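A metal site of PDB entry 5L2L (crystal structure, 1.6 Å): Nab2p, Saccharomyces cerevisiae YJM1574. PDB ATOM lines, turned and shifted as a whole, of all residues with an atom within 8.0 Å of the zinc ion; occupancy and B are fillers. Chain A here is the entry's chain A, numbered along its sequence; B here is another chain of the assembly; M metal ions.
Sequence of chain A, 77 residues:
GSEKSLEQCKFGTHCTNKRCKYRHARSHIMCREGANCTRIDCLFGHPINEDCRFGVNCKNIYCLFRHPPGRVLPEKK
O of Phe 44 sits close to ND1 of His 46. A ring nitrogen (ND1) of His 46 is in hydrogen-bond range of the side-chain amide oxygen (OE1) of Gln 8. NH2 of Arg 23 sits at hydrogen-bond distance from O of Cys 37. The side-chain sulfur (SG) of Cys 37 sits close to the backbone NH (N) of Arg 39 (3.7 Å). N of Phe 44 sits close to SG of Cys 42, at 3.6 Å. N6 of A 11 of chain B sits close to the side-chain sulfur (SG) of Cys 31, 3.5 Å away. SG of Cys 31 sits close to N of Glu 33 (3.6 Å). The backbone NH (N) of Cys 31 lies within hydrogen-bond range of the backbone carbonyl oxygen (O) of Gly 45, 2.8 Å away.
Within 4 Å of the zinc ion: Cys 31, Cys 37, Cys 42 and His 46.
The zinc ion is bound by a ring nitrogen (NE2) of His 46 (2.1 Å), the side-chain sulfur of Cys 37 (2.4 Å), the side-chain sulfur of Cys 42 (2.4 Å) and the side-chain sulfur of Cys 31 (2.4 Å). The zinc ion has four donor atoms within binding distance.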
ATOM      1  N   LEU A   6      -3.423 -22.394  -7.949  1.00  0.00           N
ATOM      2  CA  LEU A   6      -3.946 -21.355  -8.851  1.00  0.00           C
ATOM      3  C   LEU A   6      -4.993 -20.441  -8.188  1.00  0.00           C
ATOM      4  O   LEU A   6      -5.313 -19.372  -8.742  1.00  0.00           O
ATOM      5  CB  LEU A   6      -4.562 -22.000 -10.098  1.00  0.00           C
ATOM      6  CG  LEU A   6      -3.577 -22.682 -11.067  1.00  0.00           C
ATOM      7  CD1 LEU A   6      -4.327 -23.517 -12.100  1.00  0.00           C
ATOM      8  CD2 LEU A   6      -2.676 -21.671 -11.785  1.00  0.00           C
ATOM      9  N   GLN A   8      -6.658 -17.555  -6.118  1.00  0.00           N
ATOM     10  CA  GLN A   8      -6.182 -16.184  -5.930  1.00  0.00           C
ATOM     11  C   GLN A   8      -6.074 -15.816  -4.448  1.00  0.00           C
ATOM     12  O   GLN A   8      -7.023 -16.027  -3.676  1.00  0.00           O
ATOM     13  CB  GLN A   8      -7.127 -15.206  -6.631  1.00  0.00           C
ATOM     14  CG  GLN A   8      -6.541 -13.813  -6.836  1.00  0.00           C
ATOM     15  CD  GLN A   8      -5.453 -13.820  -7.897  1.00  0.00           C
ATOM     16  OE1 GLN A   8      -5.440 -14.698  -8.767  1.00  0.00           O
ATOM     17  NE2 GLN A   8      -4.547 -12.868  -7.845  1.00  0.00           N
ATOM     18  N   ARG A  23      -1.925 -17.268  -5.641  1.00  0.00           N
ATOM     19  CA  ARG A  23      -1.469 -16.298  -6.648  1.00  0.00           C
ATOM     20  C   ARG A  23      -1.689 -14.864  -6.196  1.00  0.00           C
ATOM     21  O   ARG A  23      -2.704 -14.543  -5.555  1.00  0.00           O
ATOM     22  CB  ARG A  23      -2.167 -16.548  -7.988  1.00  0.00           C
ATOM     23  CG  ARG A  23      -1.783 -17.873  -8.640  1.00  0.00           C
ATOM     24  CD  ARG A  23      -2.021 -17.863 -10.174  1.00  0.00           C
ATOM     25  NE  ARG A  23      -3.418 -18.045 -10.524  1.00  0.00           N
ATOM     26  CZ  ARG A  23      -3.860 -18.135 -11.783  1.00  0.00           C
ATOM     27  NH1 ARG A  23      -3.012 -18.051 -12.801  1.00  0.00           N
ATOM     28  NH2 ARG A  23      -5.160 -18.297 -12.020  1.00  0.00           N
ATOM     29  N   ILE A  29      -5.139  -4.566 -13.760  1.00  0.00           N
ATOM     30  CA  ILE A  29      -5.772  -5.147 -14.939  1.00  0.00           C
ATOM     31  C   ILE A  29      -6.178  -6.592 -14.642  1.00  0.00           C
ATOM     32  O   ILE A  29      -5.367  -7.388 -14.130  1.00  0.00           O
ATOM     33  CB  ILE A  29      -4.826  -5.087 -16.146  1.00  0.00           C
ATOM     34  CG1 ILE A  29      -4.566  -3.622 -16.533  1.00  0.00           C
ATOM     35  CG2 ILE A  29      -5.392  -5.914 -17.323  1.00  0.00           C
ATOM     36  CD1 ILE A  29      -3.507  -3.474 -17.541  1.00  0.00           C
ATOM     37  N   MET A  30      -7.415  -6.942 -14.988  1.00  0.00           N
ATOM     38  CA  MET A  30      -7.891  -8.305 -14.846  1.00  0.00           C
ATOM     39  C   MET A  30      -7.345  -9.181 -15.969  1.00  0.00           C
ATOM     40  O   MET A  30      -7.344  -8.778 -17.150  1.00  0.00           O
ATOM     41  CB  MET A  30      -9.422  -8.309 -14.793  1.00  0.00           C
ATOM     42  CG  MET A  30      -9.972  -7.586 -13.525  1.00  0.00           C
ATOM     43  SD  MET A  30     -11.769  -7.637 -13.381  1.00  0.00           S
ATOM     44  CE  MET A  30     -12.070  -6.473 -12.023  1.00  0.00           C
ATOM     45  N   CYS A  31      -6.835 -10.360 -15.615  1.00  0.00           N
ATOM     46  CA  CYS A  31      -6.254 -11.267 -16.598  1.00  0.00           C
ATOM     47  C   CYS A  31      -7.248 -11.571 -17.712  1.00  0.00           C
ATOM     48  O   CYS A  31      -8.414 -11.904 -17.443  1.00  0.00           O
ATOM     49  CB  CYS A  31      -5.808 -12.577 -15.932  1.00  0.00           C
ATOM     50  SG  CYS A  31      -4.932 -13.735 -17.059  1.00  0.00           S
ATOM     51  N   ARG A  32      -6.773 -11.526 -18.964  1.00  0.00           N
ATOM     52  CA  ARG A  32      -7.663 -11.752 -20.085  1.00  0.00           C
ATOM     53  C   ARG A  32      -8.199 -13.175 -20.150  1.00  0.00           C
ATOM     54  O   ARG A  32      -9.237 -13.398 -20.786  1.00  0.00           O
ATOM     55  CB  ARG A  32      -6.973 -11.382 -21.419  1.00  0.00           C
ATOM     56  CG  ARG A  32      -5.664 -12.137 -21.687  1.00  0.00           C
ATOM     57  CD  ARG A  32      -5.105 -11.896 -23.078  1.00  0.00           C
ATOM     58  NE  ARG A  32      -4.761 -10.499 -23.324  1.00  0.00           N
ATOM     59  CZ  ARG A  32      -3.536 -10.039 -23.568  1.00  0.00           C
ATOM     60  NH1 ARG A  32      -2.491 -10.860 -23.595  1.00  0.00           N
ATOM     61  NH2 ARG A  32      -3.345  -8.736 -23.780  1.00  0.00           N
ATOM     62  N   GLU A  33      -7.562 -14.138 -19.470  1.00  0.00           N
ATOM     63  CA  GLU A  33      -8.056 -15.511 -19.386  1.00  0.00           C
ATOM     64  C   GLU A  33      -8.904 -15.772 -18.142  1.00  0.00           C
ATOM     65  O   GLU A  33      -9.433 -16.890 -17.997  1.00  0.00           O
ATOM     66  CB  GLU A  33      -6.883 -16.490 -19.424  1.00  0.00           C
ATOM     67  CG  GLU A  33      -6.186 -16.547 -20.777  1.00  0.00           C
ATOM     68  CD  GLU A  33      -5.123 -17.634 -20.864  1.00  0.00           C
ATOM     69  OE1 GLU A  33      -5.332 -18.717 -20.280  1.00  0.00           O
ATOM     70  OE2 GLU A  33      -4.090 -17.402 -21.528  1.00  0.00           O
ATOM     71  N   GLY A  34      -9.053 -14.796 -17.258  1.00  0.00           N
ATOM     72  CA  GLY A  34      -9.886 -14.991 -16.077  1.00  0.00           C
ATOM     73  C   GLY A  34      -9.499 -16.190 -15.253  1.00  0.00           C
ATOM     74  O   GLY A  34      -8.309 -16.535 -15.100  1.00  0.00           O
ATOM     75  N   ALA A  35     -10.522 -16.857 -14.684  1.00  0.00           N
ATOM     76  CA  ALA A  35     -10.324 -18.041 -13.857  1.00  0.00           C
ATOM     77  C   ALA A  35      -9.793 -19.229 -14.635  1.00  0.00           C
ATOM     78  O   ALA A  35      -9.490 -20.252 -14.017  1.00  0.00           O
ATOM     79  CB  ALA A  35     -11.627 -18.427 -13.153  1.00  0.00           C
ATOM     80  N   ASN A  36      -9.668 -19.110 -15.961  1.00  0.00           N
ATOM     81  CA  ASN A  36      -9.110 -20.177 -16.791  1.00  0.00           C
ATOM     82  C   ASN A  36      -7.584 -20.132 -16.901  1.00  0.00           C
ATOM     83  O   ASN A  36      -7.000 -21.086 -17.454  1.00  0.00           O
ATOM     84  CB  ASN A  36      -9.734 -20.106 -18.184  1.00  0.00           C
ATOM     85  CG  ASN A  36     -11.245 -20.012 -18.128  1.00  0.00           C
ATOM     86  OD1 ASN A  36     -11.926 -20.987 -17.811  1.00  0.00           O
ATOM     87  ND2 ASN A  36     -11.782 -18.826 -18.425  1.00  0.00           N
ATOM     88  N   CYS A  37      -6.944 -19.090 -16.384  1.00  0.00           N
ATOM     89  CA  CYS A  37      -5.494 -18.931 -16.538  1.00  0.00           C
ATOM     90  C   CYS A  37      -4.745 -19.969 -15.694  1.00  0.00           C
ATOM     91  O   CYS A  37      -5.063 -20.164 -14.529  1.00  0.00           O
ATOM     92  CB  CYS A  37      -5.091 -17.516 -16.116  1.00  0.00           C
ATOM     93  SG  CYS A  37      -3.317 -17.152 -16.087  1.00  0.00           S
ATOM     94  N   THR A  38      -3.738 -20.621 -16.302  1.00  0.00           N
ATOM     95  CA  THR A  38      -2.986 -21.669 -15.614  1.00  0.00           C
ATOM     96  C   THR A  38      -1.533 -21.303 -15.314  1.00  0.00           C
ATOM     97  O   THR A  38      -0.744 -22.178 -14.954  1.00  0.00           O
ATOM     98  CB  THR A  38      -3.006 -22.986 -16.405  1.00  0.00           C
ATOM     99  OG1 THR A  38      -2.478 -22.804 -17.731  1.00  0.00           O
ATOM    100  CG2 THR A  38      -4.448 -23.544 -16.492  1.00  0.00           C
ATOM    101  N   ARG A  39      -1.151 -20.033 -15.439  1.00  0.00           N
ATOM    102  CA  ARG A  39       0.220 -19.580 -15.195  1.00  0.00           C
ATOM    103  C   ARG A  39       0.407 -19.277 -13.704  1.00  0.00           C
ATOM    104  O   ARG A  39      -0.173 -18.312 -13.177  1.00  0.00           O
ATOM    105  CB  ARG A  39       0.529 -18.364 -16.045  1.00  0.00           C
ATOM    106  CG  ARG A  39       1.940 -17.847 -15.867  1.00  0.00           C
ATOM    107  CD  ARG A  39       2.257 -16.701 -16.807  1.00  0.00           C
ATOM    108  NE  ARG A  39       3.622 -16.222 -16.578  1.00  0.00           N
ATOM    109  CZ  ARG A  39       4.320 -15.468 -17.428  1.00  0.00           C
ATOM    110  NH1 ARG A  39       3.779 -15.099 -18.573  1.00  0.00           N
ATOM    111  NH2 ARG A  39       5.561 -15.107 -17.109  1.00  0.00           N
ATOM    112  N   ILE A  40       1.232 -20.073 -13.025  1.00  0.00           N
ATOM    113  CA  ILE A  40       1.348 -19.991 -11.562  1.00  0.00           C
ATOM    114  C   ILE A  40       1.828 -18.599 -11.128  1.00  0.00           C
ATOM    115  O   ILE A  40       1.325 -18.047 -10.132  1.00  0.00           O
ATOM    116  CB  ILE A  40       2.280 -21.097 -11.033  1.00  0.00           C
ATOM    117  CG1 ILE A  40       1.547 -22.435 -11.005  1.00  0.00           C
ATOM    118  CG2 ILE A  40       2.816 -20.762  -9.612  1.00  0.00           C
ATOM    119  CD1 ILE A  40       0.443 -22.549  -9.924  1.00  0.00           C
ATOM    120  N   ASP A  41       2.786 -18.019 -11.860  1.00  0.00           N
ATOM    121  CA  ASP A  41       3.350 -16.722 -11.504  1.00  0.00           C
ATOM    122  C   ASP A  41       2.670 -15.549 -12.220  1.00  0.00           C
ATOM    123  O   ASP A  41       3.209 -14.423 -12.203  1.00  0.00           O
ATOM    124  CB  ASP A  41       4.876 -16.734 -11.735  1.00  0.00           C
ATOM    125  CG  ASP A  41       5.277 -16.674 -13.213  1.00  0.00           C
ATOM    126  OD1 ASP A  41       4.475 -16.991 -14.112  1.00  0.00           O
ATOM    127  OD2 ASP A  41       6.450 -16.298 -13.466  1.00  0.00           O
ATOM    128  N   CYS A  42       1.470 -15.744 -12.780  1.00  0.00           N
ATOM    129  CA  CYS A  42       0.769 -14.646 -13.443  1.00  0.00           C
ATOM    130  C   CYS A  42       0.514 -13.471 -12.492  1.00  0.00           C
ATOM    131  O   CYS A  42       0.018 -13.652 -11.376  1.00  0.00           O
ATOM    132  CB  CYS A  42      -0.575 -15.131 -14.020  1.00  0.00           C
ATOM    133  SG  CYS A  42      -1.441 -13.867 -15.046  1.00  0.00           S
ATOM    134  N   LEU A  43       0.818 -12.257 -12.961  1.00  0.00           N
ATOM    135  CA  LEU A  43       0.711 -11.056 -12.116  1.00  0.00           C
ATOM    136  C   LEU A  43      -0.595 -10.281 -12.320  1.00  0.00           C
ATOM    137  O   LEU A  43      -0.813  -9.262 -11.628  1.00  0.00           O
ATOM    138  CB  LEU A  43       1.927 -10.146 -12.364  1.00  0.00           C
ATOM    139  CG  LEU A  43       2.188  -9.488 -13.728  1.00  0.00           C
ATOM    140  CD1 LEU A  43       1.238  -8.312 -14.020  1.00  0.00           C
ATOM    141  CD2 LEU A  43       3.668  -9.011 -13.833  1.00  0.00           C
ATOM    142  N   PHE A  44      -1.467 -10.710 -13.231  1.00  0.00           N
ATOM    143  CA  PHE A  44      -2.742 -10.039 -13.455  1.00  0.00           C
ATOM    144  C   PHE A  44      -3.834 -10.592 -12.536  1.00  0.00           C
ATOM    145  O   PHE A  44      -3.686 -11.652 -11.923  1.00  0.00           O
ATOM    146  CB  PHE A  44      -3.140 -10.148 -14.945  1.00  0.00           C
ATOM    147  CG  PHE A  44      -2.179  -9.413 -15.855  1.00  0.00           C
ATOM    148  CD1 PHE A  44      -2.307  -8.046 -16.069  1.00  0.00           C
ATOM    149  CD2 PHE A  44      -1.117 -10.077 -16.474  1.00  0.00           C
ATOM    150  CE1 PHE A  44      -1.416  -7.367 -16.893  1.00  0.00           C
ATOM    151  CE2 PHE A  44      -0.224  -9.401 -17.284  1.00  0.00           C
ATOM    152  CZ  PHE A  44      -0.368  -8.045 -17.498  1.00  0.00           C
ATOM    153  N   GLY A  45      -4.929  -9.856 -12.401  1.00  0.00           N
ATOM    154  CA  GLY A  45      -5.971 -10.266 -11.444  1.00  0.00           C
ATOM    155  C   GLY A  45      -6.850 -11.416 -11.945  1.00  0.00           C
ATOM    156  O   GLY A  45      -7.221 -11.468 -13.120  1.00  0.00           O
ATOM    157  N   HIS A  46      -7.209 -12.318 -11.035  1.00  0.00           N
ATOM    158  CA  HIS A  46      -8.162 -13.387 -11.309  1.00  0.00           C
ATOM    159  C   HIS A  46      -9.250 -13.379 -10.248  1.00  0.00           C
ATOM    160  O   HIS A  46      -9.035 -12.876  -9.136  1.00  0.00           O
ATOM    161  CB  HIS A  46      -7.473 -14.777 -11.351  1.00  0.00           C
ATOM    162  CG  HIS A  46      -6.201 -14.800 -12.152  1.00  0.00           C
ATOM    163  ND1 HIS A  46      -4.970 -14.598 -11.573  1.00  0.00           N
ATOM    164  CD2 HIS A  46      -5.983 -14.968 -13.481  1.00  0.00           C
ATOM    165  CE1 HIS A  46      -4.036 -14.641 -12.514  1.00  0.00           C
ATOM    166  NE2 HIS A  46      -4.622 -14.856 -13.674  1.00  0.00           N
ATOM    167  P     A B  10       8.080  -7.842 -20.764  1.00  0.00           P
ATOM    168  OP1   A B  10       9.513  -8.097 -20.476  1.00  0.00           O
ATOM    169  OP2   A B  10       7.766  -7.054 -21.987  1.00  0.00           O
ATOM    170  O5'   A B  10       7.232  -9.191 -20.822  1.00  0.00           O
ATOM    171  C5'   A B  10       6.783  -9.761 -22.044  1.00  0.00           C
ATOM    172  C4'   A B  10       5.318 -10.135 -21.985  1.00  0.00           C
ATOM    173  O4'   A B  10       5.093 -11.091 -20.903  1.00  0.00           O
ATOM    174  C3'   A B  10       4.334  -8.984 -21.743  1.00  0.00           C
ATOM    175  O3'   A B  10       3.150  -9.226 -22.484  1.00  0.00           O
ATOM    176  C2'   A B  10       4.043  -9.083 -20.247  1.00  0.00           C
ATOM    177  O2'   A B  10       2.808  -8.527 -19.835  1.00  0.00           O
ATOM    178  C1'   A B  10       4.087 -10.596 -20.021  1.00  0.00           C
ATOM    179  N9    A B  10       4.442 -10.987 -18.669  1.00  0.00           N
ATOM    180  C8    A B  10       5.658 -10.814 -18.057  1.00  0.00           C
ATOM    181  N7    A B  10       5.693 -11.270 -16.828  1.00  0.00           N
ATOM    182  C5    A B  10       4.417 -11.782 -16.610  1.00  0.00           C
ATOM    183  C6    A B  10       3.814 -12.399 -15.497  1.00  0.00           C
ATOM    184  N6    A B  10       4.423 -12.636 -14.327  1.00  0.00           N
ATOM    185  N1    A B  10       2.527 -12.776 -15.614  1.00  0.00           N
ATOM    186  C2    A B  10       1.893 -12.556 -16.783  1.00  0.00           C
ATOM    187  N3    A B  10       2.354 -11.995 -17.900  1.00  0.00           N
ATOM    188  C4    A B  10       3.640 -11.616 -17.739  1.00  0.00           C
ATOM    189  P     A B  11       2.871  -8.460 -23.871  1.00  0.00           P
ATOM    190  OP1   A B  11       2.180  -9.417 -24.756  1.00  0.00           O
ATOM    191  OP2   A B  11       4.167  -7.858 -24.359  1.00  0.00           O
ATOM    192  O5'   A B  11       1.883  -7.296 -23.405  1.00  0.00           O
ATOM    193  C5'   A B  11       1.114  -6.500 -24.298  1.00  0.00           C
ATOM    194  C4'   A B  11       0.020  -5.767 -23.549  1.00  0.00           C
ATOM    195  O4'   A B  11      -0.939  -6.734 -23.033  1.00  0.00           O
ATOM    196  C3'   A B  11       0.493  -4.962 -22.332  1.00  0.00           C
ATOM    197  O3'   A B  11      -0.397  -3.863 -22.116  1.00  0.00           O
ATOM    198  C2'   A B  11       0.342  -5.972 -21.200  1.00  0.00           C
ATOM    199  O2'   A B  11       0.285  -5.415 -19.908  1.00  0.00           O
ATOM    200  C1'   A B  11      -0.969  -6.649 -21.604  1.00  0.00           C
ATOM    201  N9    A B  11      -1.141  -8.007 -21.070  1.00  0.00           N
ATOM    202  C8    A B  11      -0.224  -9.052 -21.096  1.00  0.00           C
ATOM    203  N7    A B  11      -0.674 -10.171 -20.569  1.00  0.00           N
ATOM    204  C5    A B  11      -1.973  -9.862 -20.171  1.00  0.00           C
ATOM    205  C6    A B  11      -2.985 -10.636 -19.546  1.00  0.00           C
ATOM    206  N6    A B  11      -2.814 -11.919 -19.175  1.00  0.00           N
ATOM    207  N1    A B  11      -4.174 -10.045 -19.288  1.00  0.00           N
ATOM    208  C2    A B  11      -4.328  -8.750 -19.659  1.00  0.00           C
ATOM    209  N3    A B  11      -3.467  -7.929 -20.250  1.00  0.00           N
ATOM    210  C4    A B  11      -2.288  -8.541 -20.489  1.00  0.00           C
HETATM  211 ZN    ZN M   1      -3.524 -14.880 -15.487  1.00  0.00          ZN
